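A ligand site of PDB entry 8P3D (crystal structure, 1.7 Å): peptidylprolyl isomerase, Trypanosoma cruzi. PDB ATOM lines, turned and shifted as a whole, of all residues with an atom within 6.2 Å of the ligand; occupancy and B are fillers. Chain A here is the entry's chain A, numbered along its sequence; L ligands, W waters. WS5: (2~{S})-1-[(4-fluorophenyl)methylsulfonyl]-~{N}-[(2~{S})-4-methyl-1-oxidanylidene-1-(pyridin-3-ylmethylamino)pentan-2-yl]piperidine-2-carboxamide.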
ATOM      1  N   TYR A  59       2.268  17.324  30.702  1.00  0.00           N
ATOM      2  CA  TYR A  59       2.607  17.473  29.301  1.00  0.00           C
ATOM      3  C   TYR A  59       4.057  17.896  29.101  1.00  0.00           C
ATOM      4  O   TYR A  59       4.705  18.420  30.005  1.00  0.00           O
ATOM      5  CB  TYR A  59       1.722  18.504  28.629  1.00  0.00           C
ATOM      6  CG  TYR A  59       1.978  19.911  29.091  1.00  0.00           C
ATOM      7  CD1 TYR A  59       1.423  20.383  30.251  1.00  0.00           C
ATOM      8  CD2 TYR A  59       2.857  20.744  28.407  1.00  0.00           C
ATOM      9  CE1 TYR A  59       1.623  21.633  30.673  1.00  0.00           C
ATOM     10  CE2 TYR A  59       3.062  22.038  28.824  1.00  0.00           C
ATOM     11  CZ  TYR A  59       2.475  22.463  30.007  1.00  0.00           C
ATOM     12  OH  TYR A  59       2.695  23.743  30.438  1.00  0.00           O
ATOM     13  N   GLY A  61       5.943  19.765  25.732  1.00  0.00           N
ATOM     14  CA  GLY A  61       5.842  20.364  24.403  1.00  0.00           C
ATOM     15  C   GLY A  61       7.217  20.497  23.750  1.00  0.00           C
ATOM     16  O   GLY A  61       8.131  21.047  24.345  1.00  0.00           O
ATOM     17  N   PHE A  69      10.037  23.253  24.779  1.00  0.00           N
ATOM     18  CA  PHE A  69       9.751  24.629  25.128  1.00  0.00           C
ATOM     19  C   PHE A  69       8.972  24.755  26.425  1.00  0.00           C
ATOM     20  O   PHE A  69       8.990  25.839  27.004  1.00  0.00           O
ATOM     21  CB  PHE A  69       9.004  25.386  23.979  1.00  0.00           C
ATOM     22  CG  PHE A  69       7.743  24.690  23.461  1.00  0.00           C
ATOM     23  CD1 PHE A  69       6.531  24.832  24.122  1.00  0.00           C
ATOM     24  CD2 PHE A  69       7.783  23.922  22.305  1.00  0.00           C
ATOM     25  CE1 PHE A  69       5.454  24.167  23.706  1.00  0.00           C
ATOM     26  CE2 PHE A  69       6.706  23.283  21.858  1.00  0.00           C
ATOM     27  CZ  PHE A  69       5.531  23.371  22.521  1.00  0.00           C
ATOM     28  N   ASP A  70       8.300  23.693  26.892  1.00  0.00           N
ATOM     29  CA  ASP A  70       7.618  23.723  28.172  1.00  0.00           C
ATOM     30  C   ASP A  70       7.268  22.317  28.603  1.00  0.00           C
ATOM     31  O   ASP A  70       7.114  21.437  27.759  1.00  0.00           O
ATOM     32  CB  ASP A  70       6.353  24.560  28.126  1.00  0.00           C
ATOM     33  CG  ASP A  70       5.959  25.074  29.511  1.00  0.00           C
ATOM     34  OD1 ASP A  70       6.858  25.506  30.243  1.00  0.00           O
ATOM     35  OD2 ASP A  70       4.765  25.038  29.831  1.00  0.00           O
ATOM     36  N   SER A  71       7.256  22.090  29.925  1.00  0.00           N
ATOM     37  CA  SER A  71       7.023  20.733  30.404  1.00  0.00           C
ATOM     38  C   SER A  71       6.578  20.803  31.853  1.00  0.00           C
ATOM     39  O   SER A  71       7.327  21.281  32.705  1.00  0.00           O
ATOM     40  CB  SER A  71       8.257  19.868  30.288  1.00  0.00           C
ATOM     41  OG  SER A  71       8.033  18.602  30.899  1.00  0.00           O
ATOM     42  N   THR A  80      -3.326  22.455  35.418  1.00  0.00           N
ATOM     43  CA  THR A  80      -4.755  22.385  35.169  1.00  0.00           C
ATOM     44  C   THR A  80      -5.178  23.463  34.197  1.00  0.00           C
ATOM     45  O   THR A  80      -4.891  24.646  34.417  1.00  0.00           O
ATOM     46  CB  THR A  80      -5.549  22.528  36.477  1.00  0.00           C
ATOM     47  OG1 THR A  80      -5.171  21.486  37.358  1.00  0.00           O
ATOM     48  CG2 THR A  80      -7.035  22.431  36.210  1.00  0.00           C
ATOM     49  N   PHE A  81      -5.846  23.057  33.123  1.00  0.00           N
ATOM     50  CA  PHE A  81      -6.340  23.941  32.093  1.00  0.00           C
ATOM     51  C   PHE A  81      -7.802  23.631  31.818  1.00  0.00           C
ATOM     52  O   PHE A  81      -8.243  22.491  31.985  1.00  0.00           O
ATOM     53  CB  PHE A  81      -5.566  23.793  30.720  1.00  0.00           C
ATOM     54  CG  PHE A  81      -4.081  23.881  30.836  1.00  0.00           C
ATOM     55  CD1 PHE A  81      -3.478  25.065  31.169  1.00  0.00           C
ATOM     56  CD2 PHE A  81      -3.281  22.771  30.567  1.00  0.00           C
ATOM     57  CE1 PHE A  81      -2.110  25.140  31.278  1.00  0.00           C
ATOM     58  CE2 PHE A  81      -1.934  22.836  30.682  1.00  0.00           C
ATOM     59  CZ  PHE A  81      -1.331  24.020  31.015  1.00  0.00           C
ATOM     60  N   GLU A  85      -9.144  27.584  27.286  1.00  0.00           N
ATOM     61  CA  GLU A  85      -8.052  28.473  27.643  1.00  0.00           C
ATOM     62  C   GLU A  85      -6.791  28.187  26.850  1.00  0.00           C
ATOM     63  O   GLU A  85      -5.826  28.931  27.003  1.00  0.00           O
ATOM     64  CB  GLU A  85      -7.715  28.353  29.135  1.00  0.00           C
ATOM     65  CG  GLU A  85      -8.855  28.731  30.063  1.00  0.00           C
ATOM     66  CD  GLU A  85      -8.504  28.426  31.536  1.00  0.00           C
ATOM     67  OE1 GLU A  85      -8.135  27.274  31.863  1.00  0.00           O
ATOM     68  OE2 GLU A  85      -8.600  29.342  32.378  1.00  0.00           O
ATOM     69  N   VAL A  86      -6.781  27.151  26.015  1.00  0.00           N
ATOM     70  CA  VAL A  86      -5.558  26.632  25.406  1.00  0.00           C
ATOM     71  C   VAL A  86      -5.665  26.733  23.890  1.00  0.00           C
ATOM     72  O   VAL A  86      -6.713  27.022  23.329  1.00  0.00           O
ATOM     73  CB  VAL A  86      -5.277  25.184  25.855  1.00  0.00           C
ATOM     74  CG1 VAL A  86      -4.800  25.214  27.304  1.00  0.00           C
ATOM     75  CG2 VAL A  86      -6.496  24.355  25.714  1.00  0.00           C
ATOM     76  N   ILE A  87      -4.519  26.507  23.215  1.00  0.00           N
ATOM     77  CA  ILE A  87      -4.497  26.571  21.756  1.00  0.00           C
ATOM     78  C   ILE A  87      -5.459  25.571  21.136  1.00  0.00           C
ATOM     79  O   ILE A  87      -5.839  24.590  21.756  1.00  0.00           O
ATOM     80  CB  ILE A  87      -3.083  26.320  21.197  1.00  0.00           C
ATOM     81  CG1 ILE A  87      -2.524  25.011  21.742  1.00  0.00           C
ATOM     82  CG2 ILE A  87      -2.178  27.420  21.521  1.00  0.00           C
ATOM     83  CD1 ILE A  87      -1.114  24.688  21.179  1.00  0.00           C
ATOM     84  N   LYS A  88      -5.853  25.840  19.882  1.00  0.00           N
ATOM     85  CA  LYS A  88      -6.965  25.109  19.264  1.00  0.00           C
ATOM     86  C   LYS A  88      -6.715  23.611  19.185  1.00  0.00           C
ATOM     87  O   LYS A  88      -7.634  22.800  19.365  1.00  0.00           O
ATOM     88  CB  LYS A  88      -7.220  25.659  17.857  1.00  0.00           C
ATOM     89  CG  LYS A  88      -7.705  27.098  17.830  1.00  0.00           C
ATOM     90  CD  LYS A  88      -7.815  27.617  16.388  1.00  0.00           C
ATOM     91  CE  LYS A  88      -7.624  29.140  16.350  1.00  0.00           C
ATOM     92  NZ  LYS A  88      -6.151  29.529  16.344  1.00  0.00           N
ATOM     93  N   TRP A  90      -5.144  21.794  21.280  1.00  0.00           N
ATOM     94  CA  TRP A  90      -5.415  21.250  22.596  1.00  0.00           C
ATOM     95  C   TRP A  90      -6.910  21.278  22.911  1.00  0.00           C
ATOM     96  O   TRP A  90      -7.427  20.315  23.464  1.00  0.00           O
ATOM     97  CB  TRP A  90      -4.682  22.039  23.637  1.00  0.00           C
ATOM     98  CG  TRP A  90      -3.298  21.526  23.972  1.00  0.00           C
ATOM     99  CD1 TRP A  90      -2.210  21.577  23.203  1.00  0.00           C
ATOM    100  CD2 TRP A  90      -2.911  20.864  25.195  1.00  0.00           C
ATOM    101  NE1 TRP A  90      -1.127  20.958  23.852  1.00  0.00           N
ATOM    102  CE2 TRP A  90      -1.532  20.573  25.101  1.00  0.00           C
ATOM    103  CE3 TRP A  90      -3.608  20.524  26.366  1.00  0.00           C
ATOM    104  CZ2 TRP A  90      -0.850  19.934  26.105  1.00  0.00           C
ATOM    105  CZ3 TRP A  90      -2.914  19.909  27.388  1.00  0.00           C
ATOM    106  CH2 TRP A  90      -1.524  19.652  27.253  1.00  0.00           C
ATOM    107  N   ALA A 112      -2.064  26.179  16.479  1.00  0.00           N
ATOM    108  CA  ALA A 112      -1.129  26.371  17.569  1.00  0.00           C
ATOM    109  C   ALA A 112      -0.915  27.866  17.695  1.00  0.00           C
ATOM    110  O   ALA A 112      -1.888  28.578  17.987  1.00  0.00           O
ATOM    111  CB  ALA A 112       0.149  25.551  17.386  1.00  0.00           C
ATOM    112  N   TYR A 113       0.302  28.359  17.567  1.00  0.00           N
ATOM    113  CA  TYR A 113       0.597  29.788  17.729  1.00  0.00           C
ATOM    114  C   TYR A 113       0.705  30.528  16.391  1.00  0.00           C
ATOM    115  O   TYR A 113       1.064  31.712  16.348  1.00  0.00           O
ATOM    116  CB  TYR A 113       1.866  29.968  18.575  1.00  0.00           C
ATOM    117  CG  TYR A 113       1.549  29.573  20.030  1.00  0.00           C
ATOM    118  CD1 TYR A 113       0.814  30.406  20.861  1.00  0.00           C
ATOM    119  CD2 TYR A 113       1.927  28.342  20.535  1.00  0.00           C
ATOM    120  CE1 TYR A 113       0.511  30.039  22.107  1.00  0.00           C
ATOM    121  CE2 TYR A 113       1.584  27.979  21.813  1.00  0.00           C
ATOM    122  CZ  TYR A 113       0.934  28.852  22.623  1.00  0.00           C
ATOM    123  OH  TYR A 113       0.537  28.488  23.906  1.00  0.00           O
ATOM    124  N   GLY A 118       4.991  32.097  19.549  1.00  0.00           N
ATOM    125  CA  GLY A 118       4.709  32.434  20.933  1.00  0.00           C
ATOM    126  C   GLY A 118       5.859  32.125  21.858  1.00  0.00           C
ATOM    127  O   GLY A 118       6.698  31.276  21.571  1.00  0.00           O
ATOM    128  N   GLY A 119       5.909  32.830  22.992  1.00  0.00           N
ATOM    129  CA  GLY A 119       6.836  32.531  24.061  1.00  0.00           C
ATOM    130  C   GLY A 119       8.268  32.807  23.756  1.00  0.00           C
ATOM    131  O   GLY A 119       9.131  32.468  24.572  1.00  0.00           O
ATOM    132  N   GLY A 120       8.561  33.390  22.600  1.00  0.00           N
ATOM    133  CA  GLY A 120       9.936  33.646  22.248  1.00  0.00           C
ATOM    134  C   GLY A 120      10.620  32.409  21.666  1.00  0.00           C
ATOM    135  O   GLY A 120      11.547  32.509  20.863  1.00  0.00           O
ATOM    136  N   MET A 121      10.186  31.226  22.093  1.00  0.00           N
ATOM    137  CA  MET A 121      10.815  29.983  21.664  1.00  0.00           C
ATOM    138  C   MET A 121      10.109  29.341  20.474  1.00  0.00           C
ATOM    139  O   MET A 121      10.747  28.520  19.794  1.00  0.00           O
ATOM    140  CB  MET A 121      10.819  28.958  22.821  1.00  0.00           C
ATOM    141  CG  MET A 121      11.715  29.306  23.884  1.00  0.00           C
ATOM    142  SD  MET A 121      11.865  27.895  25.000  1.00  0.00           S
ATOM    143  CE  MET A 121      12.894  26.776  24.097  1.00  0.00           C
ATOM    144  N   ILE A 122       8.832  29.632  20.222  1.00  0.00           N
ATOM    145  CA  ILE A 122       8.112  29.016  19.116  1.00  0.00           C
ATOM    146  C   ILE A 122       8.078  30.012  17.954  1.00  0.00           C
ATOM    147  O   ILE A 122       7.341  31.005  18.039  1.00  0.00           O
ATOM    148  CB  ILE A 122       6.691  28.605  19.527  1.00  0.00           C
ATOM    149  CG1 ILE A 122       6.766  27.602  20.710  1.00  0.00           C
ATOM    150  CG2 ILE A 122       5.978  28.010  18.377  1.00  0.00           C
ATOM    151  CD1 ILE A 122       5.392  27.186  21.204  1.00  0.00           C
ATOM    152  N   LEU A 128       3.686  21.824  16.401  1.00  0.00           N
ATOM    153  CA  LEU A 128       4.106  21.464  17.752  1.00  0.00           C
ATOM    154  C   LEU A 128       3.820  20.006  18.050  1.00  0.00           C
ATOM    155  O   LEU A 128       2.848  19.414  17.567  1.00  0.00           O
ATOM    156  CB  LEU A 128       3.418  22.312  18.837  1.00  0.00           C
ATOM    157  CG  LEU A 128       3.470  23.848  18.605  1.00  0.00           C
ATOM    158  CD1 LEU A 128       2.599  24.532  19.792  1.00  0.00           C
ATOM    159  CD2 LEU A 128       4.833  24.347  18.603  1.00  0.00           C
ATOM    160  N   PHE A 130       3.216  17.474  21.305  1.00  0.00           N
ATOM    161  CA  PHE A 130       3.013  17.363  22.750  1.00  0.00           C
ATOM    162  C   PHE A 130       2.800  15.907  23.137  1.00  0.00           C
ATOM    163  O   PHE A 130       2.136  15.163  22.436  1.00  0.00           O
ATOM    164  CB  PHE A 130       1.777  18.148  23.220  1.00  0.00           C
ATOM    165  CG  PHE A 130       1.917  19.633  23.183  1.00  0.00           C
ATOM    166  CD1 PHE A 130       1.640  20.346  22.012  1.00  0.00           C
ATOM    167  CD2 PHE A 130       2.273  20.329  24.336  1.00  0.00           C
ATOM    168  CE1 PHE A 130       1.769  21.746  22.010  1.00  0.00           C
ATOM    169  CE2 PHE A 130       2.354  21.712  24.333  1.00  0.00           C
ATOM    170  CZ  PHE A 130       2.074  22.403  23.163  1.00  0.00           C
HETATM  171  N1  WS5 L   1       0.896  25.489  26.321  1.00  0.00           N
HETATM  172  N3  WS5 L   1      -3.328  30.081  25.568  1.00  0.00           N
HETATM  173  C4  WS5 L   1       4.077  27.940  25.678  1.00  0.00           C
HETATM  174  C5  WS5 L   1       2.695  27.486  26.070  1.00  0.00           C
HETATM  175  C6  WS5 L   1      -0.230  25.678  25.447  1.00  0.00           C
HETATM  176  C7  WS5 L   1      -1.291  26.679  25.747  1.00  0.00           C
HETATM  177  C8  WS5 L   1      -1.953  28.585  26.936  1.00  0.00           C
HETATM  178  C10 WS5 L   1      -1.772  28.559  29.544  1.00  0.00           C
HETATM  179  C13 WS5 L   1      -2.093  29.622  25.820  1.00  0.00           C
HETATM  180  C15 WS5 L   1      -3.854  30.956  23.314  1.00  0.00           C
HETATM  181  C17 WS5 L   1      -4.371  30.433  20.694  1.00  0.00           C
HETATM  182  C20 WS5 L   1      -0.896  24.297  25.302  1.00  0.00           C
HETATM  183  C21 WS5 L   1      -1.290  23.721  26.680  1.00  0.00           C
HETATM  184  C22 WS5 L   1      -0.054  23.628  27.563  1.00  0.00           C
HETATM  185  C24 WS5 L   1       5.178  27.710  26.487  1.00  0.00           C
HETATM  186  C1  WS5 L   1       6.587  28.702  24.881  1.00  0.00           C
HETATM  187  C11 WS5 L   1      -1.194  29.341  30.714  1.00  0.00           C
HETATM  188  C12 WS5 L   1      -3.233  28.287  29.783  1.00  0.00           C
HETATM  189  C14 WS5 L   1      -3.528  31.272  24.754  1.00  0.00           C
HETATM  190  C16 WS5 L   1      -2.973  31.263  22.297  1.00  0.00           C
HETATM  191  C18 WS5 L   1      -5.291  30.090  21.637  1.00  0.00           C
HETATM  192  C19 WS5 L   1      -5.039  30.360  22.952  1.00  0.00           C
HETATM  193  C2  WS5 L   1       5.538  28.931  24.043  1.00  0.00           C
HETATM  194  C23 WS5 L   1       0.600  24.991  27.661  1.00  0.00           C
HETATM  195  C25 WS5 L   1       6.446  28.125  26.105  1.00  0.00           C
HETATM  196  C3  WS5 L   1       4.281  28.559  24.457  1.00  0.00           C
HETATM  197  C9  WS5 L   1      -1.625  29.319  28.237  1.00  0.00           C
HETATM  198  F1  WS5 L   1       7.816  29.087  24.474  1.00  0.00           F
HETATM  199  N2  WS5 L   1      -0.970  27.561  26.668  1.00  0.00           N
HETATM  200  N4  WS5 L   1      -3.204  31.023  20.991  1.00  0.00           N
HETATM  201  O1  WS5 L   1       2.340  25.625  24.314  1.00  0.00           O
HETATM  202  O2  WS5 L   1      -1.105  30.016  25.187  1.00  0.00           O
HETATM  203  O3  WS5 L   1      -2.343  26.760  25.111  1.00  0.00           O
HETATM  204  O4  WS5 L   1       3.262  24.967  26.524  1.00  0.00           O
HETATM  205  S1  WS5 L   1       2.351  25.766  25.741  1.00  0.00           S
HETATM  206  O   HOH W   1       1.152  27.906  28.982  1.00  0.00           O
HETATM  207  O   HOH W   2      -4.648  28.023  18.383  1.00  0.00           O
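OH of Tyr 113 is in hydrogen-bond range of O2 of the ligand (2.6 Å). The backbone NH of Ile 87 sits at hydrogen-bond distance from an oxygen (O3) of the ligand, 2.9 Å away. A nitrogen (N3) of the ligand sits at hydrogen-bond distance from the backbone carbonyl oxygen of Glu 85 (3.1 Å).
N of Phe 69 lies within hydrogen-bond range of O of Gly 61, 2.9 Å away. OD2 of Asp 70 lies within hydrogen-bond range of OH of Tyr 59 (2.5 Å). The backbone carbonyl oxygen (O) of Asp 70 sits at hydrogen-bond distance from the backbone NH (N) of Gly 61, 2.9 Å away. The backbone carbonyl oxygen (O) of Tyr 59 lies close to the side-chain hydroxyl (OG) of Ser 71 (3.5 Å).
OH of Tyr 59 touches C23 of the ligand (3.7 Å). CE1 of Phe 69 touches O1 of the ligand (3.5 Å). Asp 70 touches the ligand. CD1 of Phe 81 touches C12 of the ligand, 3.5 Å away. Val 86 touches the ligand. Trp 90 touches the ligand. Gly 118 touches the ligand. Gly 119 touches the ligand (CA to F1, 3.6 Å). CB of Met 121 touches F1 of the ligand, at 3.4 Å. CD1 of Ile 122 touches C2 of the ligand, 3.3 Å away. Phe 130 touches the ligand. 14 residues have an atom within 4 Å of the ligand: Tyr 59, Phe 69, Asp 70, Phe 81, Glu 85, Val 86, Ile 87, Trp 90, Tyr 113, Gly 118, Gly 119, Met 121, Ile 122 and Phe 130.
Water W2 lies within hydrogen-bond range of the backbone carbonyl oxygen (O) of Ala 112 (2.8 Å) and the backbone NH (N) of Lys 88 (2.9 Å).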
